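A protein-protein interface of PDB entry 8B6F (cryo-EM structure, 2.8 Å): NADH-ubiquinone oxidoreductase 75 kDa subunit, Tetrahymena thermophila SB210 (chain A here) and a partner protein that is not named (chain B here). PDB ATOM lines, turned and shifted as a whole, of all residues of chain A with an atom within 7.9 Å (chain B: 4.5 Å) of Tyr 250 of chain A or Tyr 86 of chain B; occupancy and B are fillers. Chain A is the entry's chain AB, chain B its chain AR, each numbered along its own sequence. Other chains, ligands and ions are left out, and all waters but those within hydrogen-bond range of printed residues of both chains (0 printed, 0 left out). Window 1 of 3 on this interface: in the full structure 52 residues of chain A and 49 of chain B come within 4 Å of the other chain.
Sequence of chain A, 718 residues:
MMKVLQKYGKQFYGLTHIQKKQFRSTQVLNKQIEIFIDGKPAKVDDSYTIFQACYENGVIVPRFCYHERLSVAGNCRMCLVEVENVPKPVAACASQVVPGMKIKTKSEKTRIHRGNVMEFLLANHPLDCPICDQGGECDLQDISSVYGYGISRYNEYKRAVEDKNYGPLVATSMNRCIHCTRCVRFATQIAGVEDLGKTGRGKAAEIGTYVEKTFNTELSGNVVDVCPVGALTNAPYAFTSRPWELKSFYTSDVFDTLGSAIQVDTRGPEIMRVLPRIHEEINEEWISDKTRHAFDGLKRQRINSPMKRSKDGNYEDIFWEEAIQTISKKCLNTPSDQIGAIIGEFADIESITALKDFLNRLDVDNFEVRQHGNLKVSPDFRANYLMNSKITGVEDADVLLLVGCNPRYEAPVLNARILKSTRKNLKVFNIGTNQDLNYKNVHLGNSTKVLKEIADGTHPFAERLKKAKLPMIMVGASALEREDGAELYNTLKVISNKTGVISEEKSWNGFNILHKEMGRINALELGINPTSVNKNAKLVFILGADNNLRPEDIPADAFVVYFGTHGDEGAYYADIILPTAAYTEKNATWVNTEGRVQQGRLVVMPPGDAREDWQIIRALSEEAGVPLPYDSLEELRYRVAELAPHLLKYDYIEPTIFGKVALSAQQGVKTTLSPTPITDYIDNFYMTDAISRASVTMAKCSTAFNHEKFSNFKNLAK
Among the printed residues, merely in contact across the chains: Phe 249 of chain A with Glu 108 of chain B (3.0 Å), Tyr 250 of chain A with Gln 88 of chain B (3.1 Å), Ser 248 of chain A with Gln 88 of chain B (3.4 Å), Ser 248 of chain A with Glu 108 of chain B (3.6 Å), Tyr 250 of chain A with Ile 87 of chain B (3.6 Å), Ser 248 of chain A with Tyr 86 of chain B (3.7 Å), Tyr 250 of chain A with Tyr 86 of chain B (3.7 Å), Arg 601 of chain A with Arg 84 of chain B (3.7 Å), Phe 249 of chain A with Arg 84 of chain B (3.8 Å) and Gln 263 of chain A with Gln 88 of chain B (3.9 Å).
The side-chain hydroxyl (OH) of Tyr 86 of chain B sits at hydrogen-bond distance from the side-chain carboxylate (OE1) of Glu 108 of chain B (3.3 Å).
The backbone carbonyl oxygen (O) of Tyr 86 of chain B lies within hydrogen-bond range of the backbone NH (N) of Thr 106 of chain B (2.8 Å).
The side-chain carboxylate (OD1) of Asp 265 of chain A lies within hydrogen-bond range of the side-chain hydroxyl (OG) of Ser 248 of chain A (2.6 Å).
The backbone carbonyl oxygen of Tyr 250 of chain A lies within hydrogen-bond range of the guanidinium group of Arg 601 of chain A.
The backbone carbonyl oxygen (O) of Ile 85 of chain B sits at hydrogen-bond distance from the backbone NH (N) of Ser 156 of chain B.
O of Leu 275 of chain A lies within hydrogen-bond range of N of Gln 263 of chain A (2.8 Å).
Of the 21 printed residues of chain A, 7 touch a printed residue of chain B.
Hydrophobic or aromatic side chains of chain A within 4 Å of the printed part of chain B: Phe 249, Tyr 250 and Leu 602.
Of the 10 printed residues of chain B, 7 touch a printed residue of chain A.
Among the printed residues, 14 pairs touch across the chains.
Among the printed residues, Asp or Glu carboxylates within 4 Å of a Lys or Arg side-chain nitrogen of the other chain: Lys 247 of chain A with Glu 108 of chain B (2.7 Å).
The side-chain carboxylate (OE2) of Glu 108 of chain B is in salt-bridge range of the side-chain amino group (NZ) of Lys 247 of chain A, at 2.7 Å.
OH of Tyr 250 of chain A sits at hydrogen-bond distance from N of Asp 89 of chain B.
The guanidinium group of Arg 601 of chain A lies close to the side-chain hydroxyl of Ser 156 of chain B (3.3 Å).
The backbone carbonyl oxygen (O) of Leu 602 of chain A sits at hydrogen-bond distance from the guanidinium group (NH2) of Arg 84 of chain B, at 2.9 Å.
Printed residues of chain B within 4 Å of Tyr 250 of chain A: Tyr 86, Ile 87, Gln 88 and Asp 89.
Tyr 86 of chain B touches two residues of chain A.
Of the printed residues of chain A, Gln 88 of chain B touches Ser 248, Tyr 250 and Gln 263.
Printed residues of chain B within 4 Å of Leu 602 of chain A: Arg 84.
Of the printed residues of chain B, Gln 263 of chain A touches Gln 88.
The nearest residue of chain A that does not touch Tyr 86 of chain B is Phe 249 of chain A (4.5 Å).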
ATOM      1  N   LYS A 247      18.366 -21.116 -21.872  1.00  0.00           N
ATOM      2  CA  LYS A 247      18.928 -20.142 -20.946  1.00  0.00           C
ATOM      3  C   LYS A 247      19.382 -20.879 -19.696  1.00  0.00           C
ATOM      4  O   LYS A 247      18.627 -21.679 -19.136  1.00  0.00           O
ATOM      5  CB  LYS A 247      17.906 -19.060 -20.594  1.00  0.00           C
ATOM      6  CG  LYS A 247      18.533 -17.778 -20.072  1.00  0.00           C
ATOM      7  CD  LYS A 247      17.478 -16.729 -19.769  1.00  0.00           C
ATOM      8  CE  LYS A 247      18.108 -15.376 -19.484  1.00  0.00           C
ATOM      9  NZ  LYS A 247      19.121 -15.444 -18.396  1.00  0.00           N
ATOM     10  N   SER A 248      20.608 -20.608 -19.262  1.00  0.00           N
ATOM     11  CA  SER A 248      21.258 -21.376 -18.212  1.00  0.00           C
ATOM     12  C   SER A 248      21.325 -20.579 -16.917  1.00  0.00           C
ATOM     13  O   SER A 248      21.576 -19.371 -16.930  1.00  0.00           O
ATOM     14  CB  SER A 248      22.671 -21.764 -18.650  1.00  0.00           C
ATOM     15  OG  SER A 248      22.630 -22.507 -19.856  1.00  0.00           O
ATOM     16  N   PHE A 249      21.099 -21.267 -15.799  1.00  0.00           N
ATOM     17  CA  PHE A 249      21.201 -20.682 -14.469  1.00  0.00           C
ATOM     18  C   PHE A 249      22.076 -21.569 -13.599  1.00  0.00           C
ATOM     19  O   PHE A 249      21.917 -22.793 -13.602  1.00  0.00           O
ATOM     20  CB  PHE A 249      19.822 -20.522 -13.821  1.00  0.00           C
ATOM     21  CG  PHE A 249      18.819 -19.827 -14.693  1.00  0.00           C
ATOM     22  CD1 PHE A 249      18.082 -20.540 -15.622  1.00  0.00           C
ATOM     23  CD2 PHE A 249      18.606 -18.465 -14.578  1.00  0.00           C
ATOM     24  CE1 PHE A 249      17.155 -19.907 -16.424  1.00  0.00           C
ATOM     25  CE2 PHE A 249      17.680 -17.825 -15.377  1.00  0.00           C
ATOM     26  CZ  PHE A 249      16.953 -18.548 -16.301  1.00  0.00           C
ATOM     27  N   TYR A 250      22.997 -20.957 -12.860  1.00  0.00           N
ATOM     28  CA  TYR A 250      23.830 -21.683 -11.912  1.00  0.00           C
ATOM     29  C   TYR A 250      23.106 -21.785 -10.578  1.00  0.00           C
ATOM     30  O   TYR A 250      22.672 -20.772 -10.023  1.00  0.00           O
ATOM     31  CB  TYR A 250      25.183 -20.995 -11.719  1.00  0.00           C
ATOM     32  CG  TYR A 250      26.170 -21.197 -12.846  1.00  0.00           C
ATOM     33  CD1 TYR A 250      25.802 -21.829 -14.028  1.00  0.00           C
ATOM     34  CD2 TYR A 250      27.486 -20.778 -12.713  1.00  0.00           C
ATOM     35  CE1 TYR A 250      26.710 -22.020 -15.046  1.00  0.00           C
ATOM     36  CE2 TYR A 250      28.399 -20.964 -13.723  1.00  0.00           C
ATOM     37  CZ  TYR A 250      28.008 -21.592 -14.883  1.00  0.00           C
ATOM     38  OH  TYR A 250      28.927 -21.771 -15.883  1.00  0.00           O
ATOM     39  N   THR A 251      22.982 -23.004 -10.064  1.00  0.00           N
ATOM     40  CA  THR A 251      22.320 -23.233  -8.787  1.00  0.00           C
ATOM     41  C   THR A 251      23.018 -24.392  -8.087  1.00  0.00           C
ATOM     42  O   THR A 251      24.056 -24.881  -8.544  1.00  0.00           O
ATOM     43  CB  THR A 251      20.821 -23.492  -8.994  1.00  0.00           C
ATOM     44  OG1 THR A 251      20.179 -23.654  -7.724  1.00  0.00           O
ATOM     45  CG2 THR A 251      20.597 -24.740  -9.832  1.00  0.00           C
ATOM     46  N   SER A 252      22.447 -24.833  -6.969  1.00  0.00           N
ATOM     47  CA  SER A 252      23.014 -25.896  -6.154  1.00  0.00           C
ATOM     48  C   SER A 252      22.032 -27.054  -6.054  1.00  0.00           C
ATOM     49  O   SER A 252      20.817 -26.846  -5.981  1.00  0.00           O
ATOM     50  CB  SER A 252      23.365 -25.382  -4.755  1.00  0.00           C
ATOM     51  OG  SER A 252      23.940 -26.408  -3.965  1.00  0.00           O
ATOM     52  N   SER A 260      25.621 -30.047  -4.782  1.00  0.00           N
ATOM     53  CA  SER A 260      26.375 -30.096  -6.023  1.00  0.00           C
ATOM     54  C   SER A 260      26.102 -28.847  -6.839  1.00  0.00           C
ATOM     55  O   SER A 260      24.958 -28.396  -6.940  1.00  0.00           O
ATOM     56  CB  SER A 260      26.017 -31.339  -6.846  1.00  0.00           C
ATOM     57  OG  SER A 260      26.238 -32.524  -6.102  1.00  0.00           O
ATOM     58  N   ALA A 261      27.161 -28.296  -7.424  1.00  0.00           N
ATOM     59  CA  ALA A 261      27.054 -27.115  -8.271  1.00  0.00           C
ATOM     60  C   ALA A 261      26.549 -27.555  -9.638  1.00  0.00           C
ATOM     61  O   ALA A 261      27.254 -28.257 -10.370  1.00  0.00           O
ATOM     62  CB  ALA A 261      28.404 -26.415  -8.375  1.00  0.00           C
ATOM     63  N   ILE A 262      25.327 -27.156  -9.983  1.00  0.00           N
ATOM     64  CA  ILE A 262      24.677 -27.613 -11.202  1.00  0.00           C
ATOM     65  C   ILE A 262      24.265 -26.411 -12.038  1.00  0.00           C
ATOM     66  O   ILE A 262      24.169 -25.280 -11.557  1.00  0.00           O
ATOM     67  CB  ILE A 262      23.457 -28.511 -10.914  1.00  0.00           C
ATOM     68  CG1 ILE A 262      22.419 -27.749 -10.085  1.00  0.00           C
ATOM     69  CG2 ILE A 262      23.905 -29.775 -10.204  1.00  0.00           C
ATOM     70  CD1 ILE A 262      21.161 -28.538  -9.776  1.00  0.00           C
ATOM     71  N   GLN A 263      24.026 -26.680 -13.318  1.00  0.00           N
ATOM     72  CA  GLN A 263      23.520 -25.707 -14.274  1.00  0.00           C
ATOM     73  C   GLN A 263      22.181 -26.201 -14.796  1.00  0.00           C
ATOM     74  O   GLN A 263      22.078 -27.339 -15.265  1.00  0.00           O
ATOM     75  CB  GLN A 263      24.511 -25.511 -15.422  1.00  0.00           C
ATOM     76  CG  GLN A 263      23.988 -24.681 -16.576  1.00  0.00           C
ATOM     77  CD  GLN A 263      25.006 -24.554 -17.686  1.00  0.00           C
ATOM     78  OE1 GLN A 263      26.206 -24.709 -17.465  1.00  0.00           O
ATOM     79  NE2 GLN A 263      24.530 -24.297 -18.895  1.00  0.00           N
ATOM     80  N   VAL A 264      21.161 -25.353 -14.713  1.00  0.00           N
ATOM     81  CA  VAL A 264      19.809 -25.695 -15.141  1.00  0.00           C
ATOM     82  C   VAL A 264      19.507 -24.906 -16.406  1.00  0.00           C
ATOM     83  O   VAL A 264      19.585 -23.671 -16.412  1.00  0.00           O
ATOM     84  CB  VAL A 264      18.779 -25.396 -14.041  1.00  0.00           C
ATOM     85  CG1 VAL A 264      17.397 -25.841 -14.468  1.00  0.00           C
ATOM     86  CG2 VAL A 264      19.178 -26.070 -12.737  1.00  0.00           C
ATOM     87  N   ASP A 265      19.154 -25.617 -17.472  1.00  0.00           N
ATOM     88  CA  ASP A 265      18.847 -25.022 -18.765  1.00  0.00           C
ATOM     89  C   ASP A 265      17.342 -25.053 -18.986  1.00  0.00           C
ATOM     90  O   ASP A 265      16.711 -26.102 -18.827  1.00  0.00           O
ATOM     91  CB  ASP A 265      19.563 -25.768 -19.891  1.00  0.00           C
ATOM     92  CG  ASP A 265      21.069 -25.798 -19.706  1.00  0.00           C
ATOM     93  OD1 ASP A 265      21.620 -24.834 -19.135  1.00  0.00           O
ATOM     94  OD2 ASP A 265      21.702 -26.786 -20.131  1.00  0.00           O
ATOM     95  N   LEU A 275      22.886 -30.114 -15.734  1.00  0.00           N
ATOM     96  CA  LEU A 275      24.268 -30.504 -15.955  1.00  0.00           C
ATOM     97  C   LEU A 275      25.101 -30.142 -14.738  1.00  0.00           C
ATOM     98  O   LEU A 275      24.677 -29.334 -13.904  1.00  0.00           O
ATOM     99  CB  LEU A 275      24.856 -29.811 -17.192  1.00  0.00           C
ATOM    100  CG  LEU A 275      24.266 -30.182 -18.550  1.00  0.00           C
ATOM    101  CD1 LEU A 275      24.877 -29.318 -19.634  1.00  0.00           C
ATOM    102  CD2 LEU A 275      24.484 -31.653 -18.855  1.00  0.00           C
ATOM    103  N   PRO A 276      26.286 -30.725 -14.601  1.00  0.00           N
ATOM    104  CA  PRO A 276      27.222 -30.257 -13.578  1.00  0.00           C
ATOM    105  C   PRO A 276      27.958 -29.005 -14.031  1.00  0.00           C
ATOM    106  O   PRO A 276      27.986 -28.658 -15.213  1.00  0.00           O
ATOM    107  CB  PRO A 276      28.190 -31.433 -13.426  1.00  0.00           C
ATOM    108  CG  PRO A 276      28.196 -32.071 -14.759  1.00  0.00           C
ATOM    109  CD  PRO A 276      26.805 -31.904 -15.318  1.00  0.00           C
ATOM    110  N   ARG A 277      28.554 -28.320 -13.059  1.00  0.00           N
ATOM    111  CA  ARG A 277      29.483 -27.240 -13.349  1.00  0.00           C
ATOM    112  C   ARG A 277      30.675 -27.353 -12.410  1.00  0.00           C
ATOM    113  O   ARG A 277      30.576 -27.921 -11.320  1.00  0.00           O
ATOM    114  CB  ARG A 277      28.828 -25.857 -13.230  1.00  0.00           C
ATOM    115  CG  ARG A 277      28.172 -25.560 -11.898  1.00  0.00           C
ATOM    116  CD  ARG A 277      27.551 -24.170 -11.918  1.00  0.00           C
ATOM    117  NE  ARG A 277      26.877 -23.835 -10.670  1.00  0.00           N
ATOM    118  CZ  ARG A 277      27.455 -23.245  -9.632  1.00  0.00           C
ATOM    119  NH1 ARG A 277      28.738 -22.924  -9.645  1.00  0.00           N
ATOM    120  NH2 ARG A 277      26.728 -22.975  -8.553  1.00  0.00           N
ATOM    121  N   ILE A 278      31.807 -26.810 -12.851  1.00  0.00           N
ATOM    122  CA  ILE A 278      33.071 -27.039 -12.160  1.00  0.00           C
ATOM    123  C   ILE A 278      32.996 -26.460 -10.755  1.00  0.00           C
ATOM    124  O   ILE A 278      32.842 -25.246 -10.573  1.00  0.00           O
ATOM    125  CB  ILE A 278      34.237 -26.443 -12.954  1.00  0.00           C
ATOM    126  CG1 ILE A 278      34.341 -27.125 -14.321  1.00  0.00           C
ATOM    127  CG2 ILE A 278      35.546 -26.595 -12.183  1.00  0.00           C
ATOM    128  CD1 ILE A 278      35.333 -26.478 -15.264  1.00  0.00           C
ATOM    129  N   GLN A 599      23.634 -20.479  -2.020  1.00  0.00           N
ATOM    130  CA  GLN A 599      22.396 -19.787  -2.351  1.00  0.00           C
ATOM    131  C   GLN A 599      21.740 -20.485  -3.532  1.00  0.00           C
ATOM    132  O   GLN A 599      22.324 -20.554  -4.619  1.00  0.00           O
ATOM    133  CB  GLN A 599      22.658 -18.316  -2.672  1.00  0.00           C
ATOM    134  CG  GLN A 599      21.399 -17.527  -2.982  1.00  0.00           C
ATOM    135  CD  GLN A 599      21.670 -16.047  -3.135  1.00  0.00           C
ATOM    136  OE1 GLN A 599      22.694 -15.541  -2.679  1.00  0.00           O
ATOM    137  NE2 GLN A 599      20.748 -15.341  -3.783  1.00  0.00           N
ATOM    138  N   GLY A 600      20.534 -21.007  -3.314  1.00  0.00           N
ATOM    139  CA  GLY A 600      19.744 -21.572  -4.389  1.00  0.00           C
ATOM    140  C   GLY A 600      18.930 -20.478  -5.048  1.00  0.00           C
ATOM    141  O   GLY A 600      18.233 -19.718  -4.371  1.00  0.00           O
ATOM    142  N   ARG A 601      19.032 -20.393  -6.367  1.00  0.00           N
ATOM    143  CA  ARG A 601      18.486 -19.278  -7.121  1.00  0.00           C
ATOM    144  C   ARG A 601      17.176 -19.662  -7.799  1.00  0.00           C
ATOM    145  O   ARG A 601      16.861 -20.839  -7.983  1.00  0.00           O
ATOM    146  CB  ARG A 601      19.497 -18.797  -8.163  1.00  0.00           C
ATOM    147  CG  ARG A 601      20.847 -18.437  -7.566  1.00  0.00           C
ATOM    148  CD  ARG A 601      21.810 -17.947  -8.627  1.00  0.00           C
ATOM    149  NE  ARG A 601      23.112 -17.607  -8.068  1.00  0.00           N
ATOM    150  CZ  ARG A 601      24.081 -18.480  -7.830  1.00  0.00           C
ATOM    151  NH1 ARG A 601      23.924 -19.772  -8.074  1.00  0.00           N
ATOM    152  NH2 ARG A 601      25.239 -18.049  -7.339  1.00  0.00           N
ATOM    153  N   LEU A 602      16.413 -18.638  -8.169  1.00  0.00           N
ATOM    154  CA  LEU A 602      15.109 -18.814  -8.791  1.00  0.00           C
ATOM    155  C   LEU A 602      15.290 -18.991 -10.291  1.00  0.00           C
ATOM    156  O   LEU A 602      15.779 -18.086 -10.975  1.00  0.00           O
ATOM    157  CB  LEU A 602      14.205 -17.618  -8.493  1.00  0.00           C
ATOM    158  CG  LEU A 602      12.731 -17.688  -8.916  1.00  0.00           C
ATOM    159  CD1 LEU A 602      11.932 -16.642  -8.166  1.00  0.00           C
ATOM    160  CD2 LEU A 602      12.532 -17.495 -10.414  1.00  0.00           C
ATOM    161  N   VAL A 603      14.890 -20.152 -10.799  1.00  0.00           N
ATOM    162  CA  VAL A 603      14.924 -20.437 -12.226  1.00  0.00           C
ATOM    163  C   VAL A 603      13.578 -20.151 -12.876  1.00  0.00           C
ATOM    164  O   VAL A 603      13.500 -19.420 -13.863  1.00  0.00           O
ATOM    165  CB  VAL A 603      15.364 -21.900 -12.459  1.00  0.00           C
ATOM    166  CG1 VAL A 603      15.358 -22.232 -13.936  1.00  0.00           C
ATOM    167  CG2 VAL A 603      16.742 -22.140 -11.862  1.00  0.00           C
ATOM    168  N   ARG B  84      22.245 -10.820 -10.533  1.00  0.00           N
ATOM    169  CA  ARG B  84      23.242 -11.827 -10.197  1.00  0.00           C
ATOM    170  C   ARG B  84      24.445 -11.630 -11.102  1.00  0.00           C
ATOM    171  O   ARG B  84      24.298 -11.566 -12.326  1.00  0.00           O
ATOM    172  CB  ARG B  84      22.685 -13.240 -10.374  1.00  0.00           C
ATOM    173  CG  ARG B  84      21.323 -13.466  -9.745  1.00  0.00           C
ATOM    174  CD  ARG B  84      20.612 -14.627 -10.414  1.00  0.00           C
ATOM    175  NE  ARG B  84      19.327 -14.914  -9.790  1.00  0.00           N
ATOM    176  CZ  ARG B  84      18.492 -15.857 -10.202  1.00  0.00           C
ATOM    177  NH1 ARG B  84      18.770 -16.623 -11.243  1.00  0.00           N
ATOM    178  NH2 ARG B  84      17.347 -16.038  -9.550  1.00  0.00           N
ATOM    179  N   ILE B  85      25.630 -11.536 -10.507  1.00  0.00           N
ATOM    180  CA  ILE B  85      26.861 -11.281 -11.245  1.00  0.00           C
ATOM    181  C   ILE B  85      27.765 -12.491 -11.079  1.00  0.00           C
ATOM    182  O   ILE B  85      28.182 -12.812  -9.959  1.00  0.00           O
ATOM    183  CB  ILE B  85      27.558 -10.003 -10.756  1.00  0.00           C
ATOM    184  CG1 ILE B  85      26.635  -8.797 -10.934  1.00  0.00           C
ATOM    185  CG2 ILE B  85      28.858  -9.783 -11.512  1.00  0.00           C
ATOM    186  CD1 ILE B  85      27.136  -7.545 -10.260  1.00  0.00           C
ATOM    187  N   TYR B  86      28.068 -13.160 -12.187  1.00  0.00           N
ATOM    188  CA  TYR B  86      28.876 -14.371 -12.144  1.00  0.00           C
ATOM    189  C   TYR B  86      29.444 -14.621 -13.533  1.00  0.00           C
ATOM    190  O   TYR B  86      28.999 -14.036 -14.522  1.00  0.00           O
ATOM    191  CB  TYR B  86      28.056 -15.568 -11.657  1.00  0.00           C
ATOM    192  CG  TYR B  86      26.961 -15.996 -12.603  1.00  0.00           C
ATOM    193  CD1 TYR B  86      25.809 -15.238 -12.754  1.00  0.00           C
ATOM    194  CD2 TYR B  86      27.072 -17.171 -13.329  1.00  0.00           C
ATOM    195  CE1 TYR B  86      24.804 -15.632 -13.613  1.00  0.00           C
ATOM    196  CE2 TYR B  86      26.075 -17.574 -14.190  1.00  0.00           C
ATOM    197  CZ  TYR B  86      24.943 -16.802 -14.328  1.00  0.00           C
ATOM    198  OH  TYR B  86      23.947 -17.202 -15.185  1.00  0.00           O
ATOM    199  N   ILE B  87      30.438 -15.500 -13.595  1.00  0.00           N
ATOM    200  CA  ILE B  87      31.072 -15.868 -14.855  1.00  0.00           C
ATOM    201  C   ILE B  87      30.404 -17.131 -15.378  1.00  0.00           C
ATOM    202  O   ILE B  87      30.371 -18.158 -14.693  1.00  0.00           O
ATOM    203  CB  ILE B  87      32.588 -16.065 -14.687  1.00  0.00           C
ATOM    204  CG1 ILE B  87      33.269 -14.705 -14.507  1.00  0.00           C
ATOM    205  CG2 ILE B  87      33.176 -16.825 -15.879  1.00  0.00           C
ATOM    206  CD1 ILE B  87      34.762 -14.773 -14.322  1.00  0.00           C
ATOM    207  N   GLN B  88      29.866 -17.053 -16.592  1.00  0.00           N
ATOM    208  CA  GLN B  88      29.223 -18.189 -17.242  1.00  0.00           C
ATOM    209  C   GLN B  88      30.280 -18.947 -18.036  1.00  0.00           C
ATOM    210  O   GLN B  88      30.815 -18.431 -19.022  1.00  0.00           O
ATOM    211  CB  GLN B  88      28.088 -17.715 -18.145  1.00  0.00           C
ATOM    212  CG  GLN B  88      27.325 -18.829 -18.844  1.00  0.00           C
ATOM    213  CD  GLN B  88      26.493 -19.660 -17.889  1.00  0.00           C
ATOM    214  OE1 GLN B  88      26.419 -19.369 -16.698  1.00  0.00           O
ATOM    215  NE2 GLN B  88      25.855 -20.701 -18.413  1.00  0.00           N
ATOM    216  N   ASP B  89      30.581 -20.166 -17.607  1.00  0.00           N
ATOM    217  CA  ASP B  89      31.575 -21.001 -18.259  1.00  0.00           C
ATOM    218  C   ASP B  89      30.923 -21.871 -19.328  1.00  0.00           C
ATOM    219  O   ASP B  89      29.700 -22.006 -19.402  1.00  0.00           O
ATOM    220  CB  ASP B  89      32.292 -21.877 -17.231  1.00  0.00           C
ATOM    221  CG  ASP B  89      33.056 -21.065 -16.205  1.00  0.00           C
ATOM    222  OD1 ASP B  89      33.629 -20.021 -16.578  1.00  0.00           O
ATOM    223  OD2 ASP B  89      33.081 -21.471 -15.023  1.00  0.00           O
ATOM    224  N   TRP B 105      32.012 -11.193 -17.426  1.00  0.00           N
ATOM    225  CA  TRP B 105      31.068 -11.325 -16.326  1.00  0.00           C
ATOM    226  C   TRP B 105      29.653 -11.124 -16.848  1.00  0.00           C
ATOM    227  O   TRP B 105      29.359 -10.118 -17.500  1.00  0.00           O
ATOM    228  CB  TRP B 105      31.371 -10.312 -15.224  1.00  0.00           C
ATOM    229  CG  TRP B 105      32.664 -10.554 -14.521  1.00  0.00           C
ATOM    230  CD1 TRP B 105      33.907 -10.189 -14.943  1.00  0.00           C
ATOM    231  CD2 TRP B 105      32.845 -11.216 -13.264  1.00  0.00           C
ATOM    232  NE1 TRP B 105      34.852 -10.583 -14.029  1.00  0.00           N
ATOM    233  CE2 TRP B 105      34.225 -11.218 -12.989  1.00  0.00           C
ATOM    234  CE3 TRP B 105      31.973 -11.810 -12.347  1.00  0.00           C
ATOM    235  CZ2 TRP B 105      34.755 -11.786 -11.833  1.00  0.00           C
ATOM    236  CZ3 TRP B 105      32.499 -12.376 -11.200  1.00  0.00           C
ATOM    237  CH2 TRP B 105      33.879 -12.361 -10.952  1.00  0.00           C
ATOM    238  N   THR B 106      28.779 -12.082 -16.560  1.00  0.00           N
ATOM    239  CA  THR B 106      27.376 -12.001 -16.933  1.00  0.00           C
ATOM    240  C   THR B 106      26.560 -11.462 -15.768  1.00  0.00           C
ATOM    241  O   THR B 106      26.717 -11.911 -14.629  1.00  0.00           O
ATOM    242  CB  THR B 106      26.836 -13.372 -17.347  1.00  0.00           C
ATOM    243  OG1 THR B 106      26.671 -14.195 -16.187  1.00  0.00           O
ATOM    244  CG2 THR B 106      27.789 -14.056 -18.316  1.00  0.00           C
ATOM    245  N   GLU B 108      22.633 -11.054 -14.613  1.00  0.00           N
ATOM    246  CA  GLU B 108      21.378 -11.720 -14.916  1.00  0.00           C
ATOM    247  C   GLU B 108      20.301 -11.260 -13.949  1.00  0.00           C
ATOM    248  O   GLU B 108      20.582 -10.901 -12.803  1.00  0.00           O
ATOM    249  CB  GLU B 108      21.538 -13.244 -14.828  1.00  0.00           C
ATOM    250  CG  GLU B 108      20.296 -14.035 -15.192  1.00  0.00           C
ATOM    251  CD  GLU B 108      20.522 -15.528 -15.088  1.00  0.00           C
ATOM    252  OE1 GLU B 108      21.131 -15.968 -14.092  1.00  0.00           O
ATOM    253  OE2 GLU B 108      20.106 -16.261 -16.010  1.00  0.00           O
ATOM    254  N   SER B 156      28.596 -13.921  -7.191  1.00  0.00           N
ATOM    255  CA  SER B 156      29.078 -15.278  -6.968  1.00  0.00           C
ATOM    256  C   SER B 156      30.354 -15.464  -7.774  1.00  0.00           C
ATOM    257  O   SER B 156      30.331 -15.386  -9.007  1.00  0.00           O
ATOM    258  CB  SER B 156      28.025 -16.318  -7.357  1.00  0.00           C
ATOM    259  OG  SER B 156      27.612 -16.155  -8.699  1.00  0.00           O
